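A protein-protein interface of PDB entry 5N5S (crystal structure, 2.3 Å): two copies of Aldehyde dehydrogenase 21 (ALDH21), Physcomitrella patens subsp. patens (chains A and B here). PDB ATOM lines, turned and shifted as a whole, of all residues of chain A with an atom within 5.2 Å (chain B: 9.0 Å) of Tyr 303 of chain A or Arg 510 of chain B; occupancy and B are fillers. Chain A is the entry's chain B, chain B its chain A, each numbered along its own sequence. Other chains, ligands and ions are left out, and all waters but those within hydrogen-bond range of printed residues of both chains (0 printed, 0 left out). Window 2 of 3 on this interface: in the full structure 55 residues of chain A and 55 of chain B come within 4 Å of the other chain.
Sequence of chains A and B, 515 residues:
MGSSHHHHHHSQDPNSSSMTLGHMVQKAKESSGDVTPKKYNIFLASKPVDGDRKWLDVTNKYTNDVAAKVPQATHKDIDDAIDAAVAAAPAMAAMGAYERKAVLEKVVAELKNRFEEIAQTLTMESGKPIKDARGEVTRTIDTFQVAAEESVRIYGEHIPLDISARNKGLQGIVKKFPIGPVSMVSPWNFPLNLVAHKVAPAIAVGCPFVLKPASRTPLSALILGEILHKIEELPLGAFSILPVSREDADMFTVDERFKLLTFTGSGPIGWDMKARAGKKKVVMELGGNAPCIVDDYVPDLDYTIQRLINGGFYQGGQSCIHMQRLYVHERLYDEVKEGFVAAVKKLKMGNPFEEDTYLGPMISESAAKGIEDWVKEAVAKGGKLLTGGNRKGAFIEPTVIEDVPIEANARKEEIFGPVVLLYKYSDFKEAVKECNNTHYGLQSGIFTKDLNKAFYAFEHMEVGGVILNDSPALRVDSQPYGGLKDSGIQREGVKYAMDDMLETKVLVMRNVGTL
The backbone carbonyl oxygen of Val 508 of chain B sits at hydrogen-bond distance from the backbone NH of Leu 468 of chain A (2.8 Å).
The backbone NH (N) of Arg 510 of chain B lies within hydrogen-bond range of the backbone carbonyl oxygen (O) of Leu 468 of chain A (3.2 Å).
The side-chain carboxylate (OD2) of Asp 470 of chain A lies within salt-bridge range of the guanidinium group (NH2) of Arg 510 of chain B (2.8 Å).
O of Leu 170 of chain B sits at hydrogen-bond distance from N of Leu 161 of chain B (3.1 Å).
O of Gln 171 of chain B is in hydrogen-bond range of N of Met 509 of chain B (2.8 Å).
The backbone carbonyl oxygen (O) of Val 512 of chain B sits close to the side-chain amide oxygen (OE1) of Gln 171 of chain B.
The side-chain carboxylate (OD1) of Asp 300 of chain A lies within hydrogen-bond range of the backbone NH (N) of Tyr 303 of chain A (3.0 Å).
NH2 of Arg 307 of chain A is in salt-bridge range of OD2 of Asp 470 of chain A (2.8 Å).
Tyr 303 of chain A touches Arg 510 of chain B (OH to CD, 3.7 Å).
Arg 510 of chain B touches Arg 307 of chain A (NH2 to NH2, 3.7 Å).
Leu 468 of chain A touches Leu 507 of chain B (CB to CD1, 3.9 Å).
O of Leu 468 of chain A touches CA of Met 509 of chain B, 3.9 Å away.
CG2 of Val 512 of chain B touches CD2 of Leu 468 of chain A, 3.9 Å away.
CG of Arg 510 of chain B touches O of Asn 469 of chain A, at 3.4 Å.
CD2 of Leu 474 of chain A touches CD2 of Leu 170 of chain B, 3.9 Å away.
Leu 474 of chain A touches Val 508 of chain B (CD2 to CG1, 3.8 Å).
CD1 of Leu 474 of chain A touches NH2 of Arg 510 of chain B, at 3.8 Å.
No residue of chain B comes within 4 Å of Gln 306 of chain A.
Of the printed residues of chain A, Met 509 of chain B touches Leu 468 (3.9 Å).
Printed residues of chain A within 4 Å of Val 512 of chain B: Leu 468.
Printed residues of chain B within 4 Å of Arg 307 of chain A: Arg 510 (3.7 Å).
Printed residues of chain B within 4 Å of Leu 474 of chain A: Leu 170, Val 508 and Arg 510.
Arg 166 of chain B touches none of the printed residues of chain A.
Gln 171 of chain B touches none of the printed residues of chain A.
The nearest residue of chain B that does not touch Tyr 303 of chain A is Asn 511 of chain B (5.3 Å).
Hydrophobic or aromatic side chains of chain A within 4 Å of the printed part of chain B: Tyr 303, Leu 468 and Leu 474.
Of the 18 printed residues of chain B, 6 touch a printed residue of chain A.
Among the printed residues, Asp or Glu carboxylates within 4 Å of a Lys or Arg side-chain nitrogen of the other chain: Asp 470 of chain A with Arg 510 of chain B (2.8 Å).
No position is printed for both chains.
Of the 12 pairs that touch across the chains among the printed residues, none has its exchanged pair printed and touching as well.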
ATOM      1  N   VAL A 298      -4.355  18.809 -29.110  1.00  0.00           N
ATOM      2  CA  VAL A 298      -5.029  17.977 -30.119  1.00  0.00           C
ATOM      3  C   VAL A 298      -6.538  18.319 -30.269  1.00  0.00           C
ATOM      4  O   VAL A 298      -7.305  18.037 -29.351  1.00  0.00           O
ATOM      5  CB  VAL A 298      -4.807  16.446 -29.913  1.00  0.00           C
ATOM      6  CG1 VAL A 298      -5.157  15.670 -31.186  1.00  0.00           C
ATOM      7  CG2 VAL A 298      -3.375  16.131 -29.467  1.00  0.00           C
ATOM      8  N   PRO A 299      -6.987  18.878 -31.429  1.00  0.00           N
ATOM      9  CA  PRO A 299      -6.187  19.284 -32.608  1.00  0.00           C
ATOM     10  C   PRO A 299      -5.432  20.604 -32.416  1.00  0.00           C
ATOM     11  O   PRO A 299      -4.420  20.824 -33.083  1.00  0.00           O
ATOM     12  CB  PRO A 299      -7.238  19.359 -33.723  1.00  0.00           C
ATOM     13  CG  PRO A 299      -8.497  19.775 -33.020  1.00  0.00           C
ATOM     14  CD  PRO A 299      -8.422  19.182 -31.624  1.00  0.00           C
ATOM     15  N   ASP A 300      -5.926  21.471 -31.500  1.00  0.00           N
ATOM     16  CA  ASP A 300      -5.372  22.788 -31.159  1.00  0.00           C
ATOM     17  C   ASP A 300      -5.526  23.091 -29.664  1.00  0.00           C
ATOM     18  O   ASP A 300      -6.230  22.361 -28.963  1.00  0.00           O
ATOM     19  CB  ASP A 300      -6.033  23.897 -32.006  1.00  0.00           C
ATOM     20  CG  ASP A 300      -7.551  23.906 -31.984  1.00  0.00           C
ATOM     21  OD1 ASP A 300      -8.129  24.252 -30.932  1.00  0.00           O
ATOM     22  OD2 ASP A 300      -8.158  23.589 -33.024  1.00  0.00           O
ATOM     23  N   LEU A 301      -4.882  24.176 -29.191  1.00  0.00           N
ATOM     24  CA  LEU A 301      -4.884  24.640 -27.800  1.00  0.00           C
ATOM     25  C   LEU A 301      -6.275  24.961 -27.247  1.00  0.00           C
ATOM     26  O   LEU A 301      -6.563  24.592 -26.107  1.00  0.00           O
ATOM     27  CB  LEU A 301      -3.931  25.853 -27.645  1.00  0.00           C
ATOM     28  CG  LEU A 301      -3.847  26.531 -26.266  1.00  0.00           C
ATOM     29  CD1 LEU A 301      -3.268  25.605 -25.222  1.00  0.00           C
ATOM     30  CD2 LEU A 301      -3.029  27.794 -26.331  1.00  0.00           C
ATOM     31  N   ASP A 302      -7.118  25.663 -28.033  1.00  0.00           N
ATOM     32  CA  ASP A 302      -8.474  26.052 -27.632  1.00  0.00           C
ATOM     33  C   ASP A 302      -9.335  24.841 -27.340  1.00  0.00           C
ATOM     34  O   ASP A 302      -9.971  24.787 -26.280  1.00  0.00           O
ATOM     35  CB  ASP A 302      -9.138  26.951 -28.685  1.00  0.00           C
ATOM     36  CG  ASP A 302      -8.362  28.218 -28.995  1.00  0.00           C
ATOM     37  OD1 ASP A 302      -8.103  29.005 -28.052  1.00  0.00           O
ATOM     38  OD2 ASP A 302      -8.017  28.423 -30.176  1.00  0.00           O
ATOM     39  N   TYR A 303      -9.327  23.843 -28.260  1.00  0.00           N
ATOM     40  CA  TYR A 303     -10.091  22.611 -28.085  1.00  0.00           C
ATOM     41  C   TYR A 303      -9.581  21.832 -26.883  1.00  0.00           C
ATOM     42  O   TYR A 303     -10.398  21.323 -26.123  1.00  0.00           O
ATOM     43  CB  TYR A 303     -10.091  21.745 -29.357  1.00  0.00           C
ATOM     44  CG  TYR A 303     -11.044  20.575 -29.246  1.00  0.00           C
ATOM     45  CD1 TYR A 303     -12.416  20.749 -29.411  1.00  0.00           C
ATOM     46  CD2 TYR A 303     -10.584  19.305 -28.904  1.00  0.00           C
ATOM     47  CE1 TYR A 303     -13.305  19.680 -29.264  1.00  0.00           C
ATOM     48  CE2 TYR A 303     -11.457  18.223 -28.792  1.00  0.00           C
ATOM     49  CZ  TYR A 303     -12.820  18.417 -28.958  1.00  0.00           C
ATOM     50  OH  TYR A 303     -13.685  17.358 -28.815  1.00  0.00           O
ATOM     51  N   THR A 304      -8.242  21.754 -26.701  1.00  0.00           N
ATOM     52  CA  THR A 304      -7.598  21.051 -25.583  1.00  0.00           C
ATOM     53  C   THR A 304      -8.056  21.633 -24.239  1.00  0.00           C
ATOM     54  O   THR A 304      -8.512  20.871 -23.392  1.00  0.00           O
ATOM     55  CB  THR A 304      -6.065  21.020 -25.746  1.00  0.00           C
ATOM     56  OG1 THR A 304      -5.740  20.490 -27.034  1.00  0.00           O
ATOM     57  CG2 THR A 304      -5.376  20.194 -24.663  1.00  0.00           C
ATOM     58  N   ILE A 305      -8.007  22.972 -24.083  1.00  0.00           N
ATOM     59  CA  ILE A 305      -8.432  23.680 -22.869  1.00  0.00           C
ATOM     60  C   ILE A 305      -9.938  23.444 -22.604  1.00  0.00           C
ATOM     61  O   ILE A 305     -10.304  23.124 -21.473  1.00  0.00           O
ATOM     62  CB  ILE A 305      -7.996  25.185 -22.894  1.00  0.00           C
ATOM     63  CG1 ILE A 305      -6.832  25.444 -21.918  1.00  0.00           C
ATOM     64  CG2 ILE A 305      -9.141  26.169 -22.611  1.00  0.00           C
ATOM     65  CD1 ILE A 305      -5.471  25.050 -22.393  1.00  0.00           C
ATOM     66  N   GLN A 306     -10.772  23.521 -23.661  1.00  0.00           N
ATOM     67  CA  GLN A 306     -12.213  23.291 -23.624  1.00  0.00           C
ATOM     68  C   GLN A 306     -12.541  21.876 -23.065  1.00  0.00           C
ATOM     69  O   GLN A 306     -13.495  21.733 -22.294  1.00  0.00           O
ATOM     70  CB  GLN A 306     -12.785  23.470 -25.043  1.00  0.00           C
ATOM     71  CG  GLN A 306     -14.302  23.622 -25.126  1.00  0.00           C
ATOM     72  CD  GLN A 306     -14.888  22.941 -26.347  1.00  0.00           C
ATOM     73  OE1 GLN A 306     -15.443  21.837 -26.266  1.00  0.00           O
ATOM     74  NE2 GLN A 306     -14.758  23.574 -27.511  1.00  0.00           N
ATOM     75  N   ARG A 307     -11.727  20.854 -23.418  1.00  0.00           N
ATOM     76  CA  ARG A 307     -11.918  19.482 -22.943  1.00  0.00           C
ATOM     77  C   ARG A 307     -11.373  19.282 -21.532  1.00  0.00           C
ATOM     78  O   ARG A 307     -11.931  18.487 -20.767  1.00  0.00           O
ATOM     79  CB  ARG A 307     -11.343  18.451 -23.929  1.00  0.00           C
ATOM     80  CG  ARG A 307     -11.959  18.538 -25.320  1.00  0.00           C
ATOM     81  CD  ARG A 307     -13.144  17.610 -25.515  1.00  0.00           C
ATOM     82  NE  ARG A 307     -14.377  18.140 -24.932  1.00  0.00           N
ATOM     83  CZ  ARG A 307     -15.333  17.392 -24.388  1.00  0.00           C
ATOM     84  NH1 ARG A 307     -16.417  17.960 -23.880  1.00  0.00           N
ATOM     85  NH2 ARG A 307     -15.204  16.070 -24.330  1.00  0.00           N
ATOM     86  N   LEU A 308     -10.302  20.015 -21.184  1.00  0.00           N
ATOM     87  CA  LEU A 308      -9.692  19.978 -19.859  1.00  0.00           C
ATOM     88  C   LEU A 308     -10.649  20.619 -18.845  1.00  0.00           C
ATOM     89  O   LEU A 308     -10.760  20.123 -17.723  1.00  0.00           O
ATOM     90  CB  LEU A 308      -8.325  20.701 -19.860  1.00  0.00           C
ATOM     91  CG  LEU A 308      -7.167  20.055 -20.643  1.00  0.00           C
ATOM     92  CD1 LEU A 308      -5.944  20.960 -20.643  1.00  0.00           C
ATOM     93  CD2 LEU A 308      -6.828  18.668 -20.124  1.00  0.00           C
ATOM     94  N   LEU A 468      -7.926   8.872 -25.134  1.00  0.00           N
ATOM     95  CA  LEU A 468      -6.930   9.417 -26.041  1.00  0.00           C
ATOM     96  C   LEU A 468      -7.482  10.613 -26.808  1.00  0.00           C
ATOM     97  O   LEU A 468      -8.416  10.484 -27.604  1.00  0.00           O
ATOM     98  CB  LEU A 468      -6.407   8.309 -26.975  1.00  0.00           C
ATOM     99  CG  LEU A 468      -5.384   8.666 -28.055  1.00  0.00           C
ATOM    100  CD1 LEU A 468      -4.125   9.312 -27.464  1.00  0.00           C
ATOM    101  CD2 LEU A 468      -5.058   7.431 -28.911  1.00  0.00           C
ATOM    102  N   ASN A 469      -6.900  11.786 -26.514  1.00  0.00           N
ATOM    103  CA  ASN A 469      -7.157  13.115 -27.066  1.00  0.00           C
ATOM    104  C   ASN A 469      -8.518  13.659 -26.629  1.00  0.00           C
ATOM    105  O   ASN A 469      -9.236  14.338 -27.370  1.00  0.00           O
ATOM    106  CB  ASN A 469      -6.899  13.177 -28.571  1.00  0.00           C
ATOM    107  CG  ASN A 469      -5.432  12.970 -28.841  1.00  0.00           C
ATOM    108  OD1 ASN A 469      -4.585  13.348 -28.038  1.00  0.00           O
ATOM    109  ND2 ASN A 469      -5.091  12.315 -29.933  1.00  0.00           N
ATOM    110  N   ASP A 470      -8.793  13.413 -25.341  1.00  0.00           N
ATOM    111  CA  ASP A 470      -9.889  13.922 -24.533  1.00  0.00           C
ATOM    112  C   ASP A 470      -9.489  13.709 -23.066  1.00  0.00           C
ATOM    113  O   ASP A 470      -8.528  12.980 -22.793  1.00  0.00           O
ATOM    114  CB  ASP A 470     -11.254  13.300 -24.888  1.00  0.00           C
ATOM    115  CG  ASP A 470     -12.461  14.174 -24.555  1.00  0.00           C
ATOM    116  OD1 ASP A 470     -12.334  15.072 -23.693  1.00  0.00           O
ATOM    117  OD2 ASP A 470     -13.542  13.941 -25.137  1.00  0.00           O
ATOM    118  N   LEU A 474     -14.550  11.322 -20.186  1.00  0.00           N
ATOM    119  CA  LEU A 474     -15.347  10.811 -21.296  1.00  0.00           C
ATOM    120  C   LEU A 474     -15.796   9.359 -21.069  1.00  0.00           C
ATOM    121  O   LEU A 474     -14.975   8.501 -20.733  1.00  0.00           O
ATOM    122  CB  LEU A 474     -14.582  10.957 -22.624  1.00  0.00           C
ATOM    123  CG  LEU A 474     -15.270  10.459 -23.898  1.00  0.00           C
ATOM    124  CD1 LEU A 474     -16.504  11.281 -24.233  1.00  0.00           C
ATOM    125  CD2 LEU A 474     -14.311  10.473 -25.061  1.00  0.00           C
ATOM    126  N   LEU B 161     -17.502   3.491 -31.526  1.00  0.00           N
ATOM    127  CA  LEU B 161     -18.105   4.121 -30.356  1.00  0.00           C
ATOM    128  C   LEU B 161     -19.042   5.265 -30.722  1.00  0.00           C
ATOM    129  O   LEU B 161     -19.650   5.868 -29.832  1.00  0.00           O
ATOM    130  CB  LEU B 161     -17.041   4.541 -29.323  1.00  0.00           C
ATOM    131  CG  LEU B 161     -16.426   3.392 -28.514  1.00  0.00           C
ATOM    132  CD1 LEU B 161     -15.268   3.875 -27.676  1.00  0.00           C
ATOM    133  CD2 LEU B 161     -17.473   2.709 -27.641  1.00  0.00           C
ATOM    134  N   SER B 164     -24.216   7.104 -31.332  1.00  0.00           N
ATOM    135  CA  SER B 164     -25.149   8.224 -31.369  1.00  0.00           C
ATOM    136  C   SER B 164     -24.384   9.495 -31.769  1.00  0.00           C
ATOM    137  O   SER B 164     -23.150   9.503 -31.716  1.00  0.00           O
ATOM    138  CB  SER B 164     -25.850   8.392 -30.025  1.00  0.00           C
ATOM    139  OG  SER B 164     -24.933   8.625 -28.969  1.00  0.00           O
ATOM    140  N   ALA B 165     -25.124  10.551 -32.177  1.00  0.00           N
ATOM    141  CA  ALA B 165     -24.591  11.829 -32.648  1.00  0.00           C
ATOM    142  C   ALA B 165     -23.593  12.507 -31.704  1.00  0.00           C
ATOM    143  O   ALA B 165     -22.590  13.048 -32.185  1.00  0.00           O
ATOM    144  CB  ALA B 165     -25.725  12.777 -32.989  1.00  0.00           C
ATOM    145  N   ARG B 166     -23.841  12.474 -30.377  1.00  0.00           N
ATOM    146  CA  ARG B 166     -22.924  13.101 -29.418  1.00  0.00           C
ATOM    147  C   ARG B 166     -21.563  12.389 -29.363  1.00  0.00           C
ATOM    148  O   ARG B 166     -20.567  13.013 -28.992  1.00  0.00           O
ATOM    149  CB  ARG B 166     -23.547  13.275 -28.011  1.00  0.00           C
ATOM    150  CG  ARG B 166     -23.907  11.981 -27.298  1.00  0.00           C
ATOM    151  CD  ARG B 166     -23.620  12.057 -25.805  1.00  0.00           C
ATOM    152  NE  ARG B 166     -23.066  10.799 -25.299  1.00  0.00           N
ATOM    153  CZ  ARG B 166     -23.793   9.759 -24.902  1.00  0.00           C
ATOM    154  NH1 ARG B 166     -23.201   8.651 -24.475  1.00  0.00           N
ATOM    155  NH2 ARG B 166     -25.120   9.814 -24.940  1.00  0.00           N
ATOM    156  N   ASN B 167     -21.533  11.097 -29.748  1.00  0.00           N
ATOM    157  CA  ASN B 167     -20.329  10.269 -29.779  1.00  0.00           C
ATOM    158  C   ASN B 167     -19.640  10.210 -31.152  1.00  0.00           C
ATOM    159  O   ASN B 167     -18.786   9.349 -31.363  1.00  0.00           O
ATOM    160  CB  ASN B 167     -20.628   8.869 -29.251  1.00  0.00           C
ATOM    161  CG  ASN B 167     -21.201   8.830 -27.859  1.00  0.00           C
ATOM    162  OD1 ASN B 167     -22.313   8.358 -27.650  1.00  0.00           O
ATOM    163  ND2 ASN B 167     -20.466   9.314 -26.872  1.00  0.00           N
ATOM    164  N   LYS B 168     -19.954  11.153 -32.057  1.00  0.00           N
ATOM    165  CA  LYS B 168     -19.322  11.255 -33.374  1.00  0.00           C
ATOM    166  C   LYS B 168     -17.785  11.307 -33.242  1.00  0.00           C
ATOM    167  O   LYS B 168     -17.255  12.034 -32.392  1.00  0.00           O
ATOM    168  CB  LYS B 168     -19.833  12.518 -34.097  1.00  0.00           C
ATOM    169  CG  LYS B 168     -19.196  12.797 -35.466  1.00  0.00           C
ATOM    170  CD  LYS B 168     -19.482  14.224 -35.937  1.00  0.00           C
ATOM    171  CE  LYS B 168     -18.853  14.540 -37.274  1.00  0.00           C
ATOM    172  NZ  LYS B 168     -19.224  15.900 -37.751  1.00  0.00           N
ATOM    173  N   GLY B 169     -17.100  10.538 -34.087  1.00  0.00           N
ATOM    174  CA  GLY B 169     -15.640  10.501 -34.148  1.00  0.00           C
ATOM    175  C   GLY B 169     -14.963   9.675 -33.076  1.00  0.00           C
ATOM    176  O   GLY B 169     -13.751   9.799 -32.872  1.00  0.00           O
ATOM    177  N   LEU B 170     -15.733   8.819 -32.391  1.00  0.00           N
ATOM    178  CA  LEU B 170     -15.181   7.976 -31.343  1.00  0.00           C
ATOM    179  C   LEU B 170     -15.073   6.531 -31.775  1.00  0.00           C
ATOM    180  O   LEU B 170     -15.972   6.002 -32.425  1.00  0.00           O
ATOM    181  CB  LEU B 170     -15.958   8.111 -30.018  1.00  0.00           C
ATOM    182  CG  LEU B 170     -15.981   9.508 -29.355  1.00  0.00           C
ATOM    183  CD1 LEU B 170     -16.955   9.534 -28.187  1.00  0.00           C
ATOM    184  CD2 LEU B 170     -14.598   9.938 -28.885  1.00  0.00           C
ATOM    185  N   GLN B 171     -13.951   5.902 -31.431  1.00  0.00           N
ATOM    186  CA  GLN B 171     -13.690   4.489 -31.694  1.00  0.00           C
ATOM    187  C   GLN B 171     -12.918   3.937 -30.487  1.00  0.00           C
ATOM    188  O   GLN B 171     -12.377   4.716 -29.705  1.00  0.00           O
ATOM    189  CB  GLN B 171     -12.942   4.292 -33.038  1.00  0.00           C
ATOM    190  CG  GLN B 171     -11.438   4.507 -32.984  1.00  0.00           C
ATOM    191  CD  GLN B 171     -10.792   4.616 -34.342  1.00  0.00           C
ATOM    192  OE1 GLN B 171     -10.301   5.679 -34.741  1.00  0.00           O
ATOM    193  NE2 GLN B 171     -10.672   3.505 -35.041  1.00  0.00           N
ATOM    194  N   GLY B 172     -12.902   2.623 -30.316  1.00  0.00           N
ATOM    195  CA  GLY B 172     -12.198   2.044 -29.186  1.00  0.00           C
ATOM    196  C   GLY B 172     -11.443   0.770 -29.485  1.00  0.00           C
ATOM    197  O   GLY B 172     -11.811   0.016 -30.395  1.00  0.00           O
ATOM    198  N   LEU B 507      -9.146   1.643 -24.906  1.00  0.00           N
ATOM    199  CA  LEU B 507      -8.532   2.860 -25.383  1.00  0.00           C
ATOM    200  C   LEU B 507      -9.636   3.584 -26.158  1.00  0.00           C
ATOM    201  O   LEU B 507     -10.037   3.114 -27.211  1.00  0.00           O
ATOM    202  CB  LEU B 507      -7.288   2.584 -26.267  1.00  0.00           C
ATOM    203  CG  LEU B 507      -6.525   3.813 -26.784  1.00  0.00           C
ATOM    204  CD1 LEU B 507      -5.953   4.651 -25.639  1.00  0.00           C
ATOM    205  CD2 LEU B 507      -5.411   3.406 -27.738  1.00  0.00           C
ATOM    206  N   VAL B 508     -10.183   4.673 -25.597  1.00  0.00           N
ATOM    207  CA  VAL B 508     -11.241   5.459 -26.237  1.00  0.00           C
ATOM    208  C   VAL B 508     -10.548   6.539 -27.044  1.00  0.00           C
ATOM    209  O   VAL B 508      -9.892   7.413 -26.477  1.00  0.00           O
ATOM    210  CB  VAL B 508     -12.279   6.025 -25.232  1.00  0.00           C
ATOM    211  CG1 VAL B 508     -13.314   6.893 -25.946  1.00  0.00           C
ATOM    212  CG2 VAL B 508     -12.963   4.894 -24.456  1.00  0.00           C
ATOM    213  N   MET B 509     -10.671   6.448 -28.376  1.00  0.00           N
ATOM    214  CA  MET B 509     -10.003   7.316 -29.335  1.00  0.00           C
ATOM    215  C   MET B 509     -10.921   8.359 -29.966  1.00  0.00           C
ATOM    216  O   MET B 509     -11.896   8.025 -30.639  1.00  0.00           O
ATOM    217  CB  MET B 509      -9.315   6.471 -30.400  1.00  0.00           C
ATOM    218  CG  MET B 509      -8.467   5.357 -29.826  1.00  0.00           C
ATOM    219  SD  MET B 509      -8.225   4.028 -31.021  1.00  0.00           S
ATOM    220  CE  MET B 509      -6.764   4.592 -31.803  1.00  0.00           C
ATOM    221  N   ARG B 510     -10.583   9.628 -29.746  1.00  0.00           N
ATOM    222  CA  ARG B 510     -11.310  10.787 -30.253  1.00  0.00           C
ATOM    223  C   ARG B 510     -10.603  11.310 -31.492  1.00  0.00           C
ATOM    224  O   ARG B 510      -9.461  11.774 -31.397  1.00  0.00           O
ATOM    225  CB  ARG B 510     -11.437  11.851 -29.133  1.00  0.00           C
ATOM    226  CG  ARG B 510     -11.573  13.318 -29.557  1.00  0.00           C
ATOM    227  CD  ARG B 510     -12.994  13.807 -29.627  1.00  0.00           C
ATOM    228  NE  ARG B 510     -13.694  13.672 -28.353  1.00  0.00           N
ATOM    229  CZ  ARG B 510     -15.012  13.739 -28.230  1.00  0.00           C
ATOM    230  NH1 ARG B 510     -15.771  13.972 -29.290  1.00  0.00           N
ATOM    231  NH2 ARG B 510     -15.579  13.600 -27.041  1.00  0.00           N
ATOM    232  N   ASN B 511     -11.274  11.185 -32.660  1.00  0.00           N
ATOM    233  CA  ASN B 511     -10.832  11.625 -33.992  1.00  0.00           C
ATOM    234  C   ASN B 511      -9.386  11.234 -34.335  1.00  0.00           C
ATOM    235  O   ASN B 511      -8.621  12.048 -34.856  1.00  0.00           O
ATOM    236  CB  ASN B 511     -11.060  13.146 -34.182  1.00  0.00           C
ATOM    237  CG  ASN B 511     -12.510  13.575 -34.029  1.00  0.00           C
ATOM    238  OD1 ASN B 511     -13.450  13.026 -34.618  1.00  0.00           O
ATOM    239  ND2 ASN B 511     -12.720  14.559 -33.193  1.00  0.00           N
ATOM    240  N   VAL B 512      -9.019   9.980 -34.035  1.00  0.00           N
ATOM    241  CA  VAL B 512      -7.694   9.433 -34.342  1.00  0.00           C
ATOM    242  C   VAL B 512      -7.740   9.053 -35.817  1.00  0.00           C
ATOM    243  O   VAL B 512      -8.631   8.307 -36.227  1.00  0.00           O
ATOM    244  CB  VAL B 512      -7.286   8.256 -33.402  1.00  0.00           C
ATOM    245  CG1 VAL B 512      -6.042   7.542 -33.915  1.00  0.00           C
ATOM    246  CG2 VAL B 512      -7.051   8.758 -31.978  1.00  0.00           C
ATOM    247  N   GLY B 513      -6.844   9.650 -36.600  1.00  0.00           N
ATOM    248  CA  GLY B 513      -6.794   9.447 -38.042  1.00  0.00           C
ATOM    249  C   GLY B 513      -7.193  10.692 -38.805  1.00  0.00           C
ATOM    250  O   GLY B 513      -7.239  10.678 -40.040  1.00  0.00           O
ATOM    251  N   THR B 514      -7.512  11.773 -38.059  1.00  0.00           N
ATOM    252  CA  THR B 514      -7.879  13.076 -38.600  1.00  0.00           C
ATOM    253  C   THR B 514      -6.575  13.858 -38.736  1.00  0.00           C
ATOM    254  O   THR B 514      -5.911  14.127 -37.726  1.00  0.00           O
ATOM    255  CB  THR B 514      -8.940  13.757 -37.688  1.00  0.00           C
ATOM    256  OG1 THR B 514     -10.126  12.950 -37.638  1.00  0.00           O
ATOM    257  CG2 THR B 514      -9.286  15.182 -38.124  1.00  0.00           C
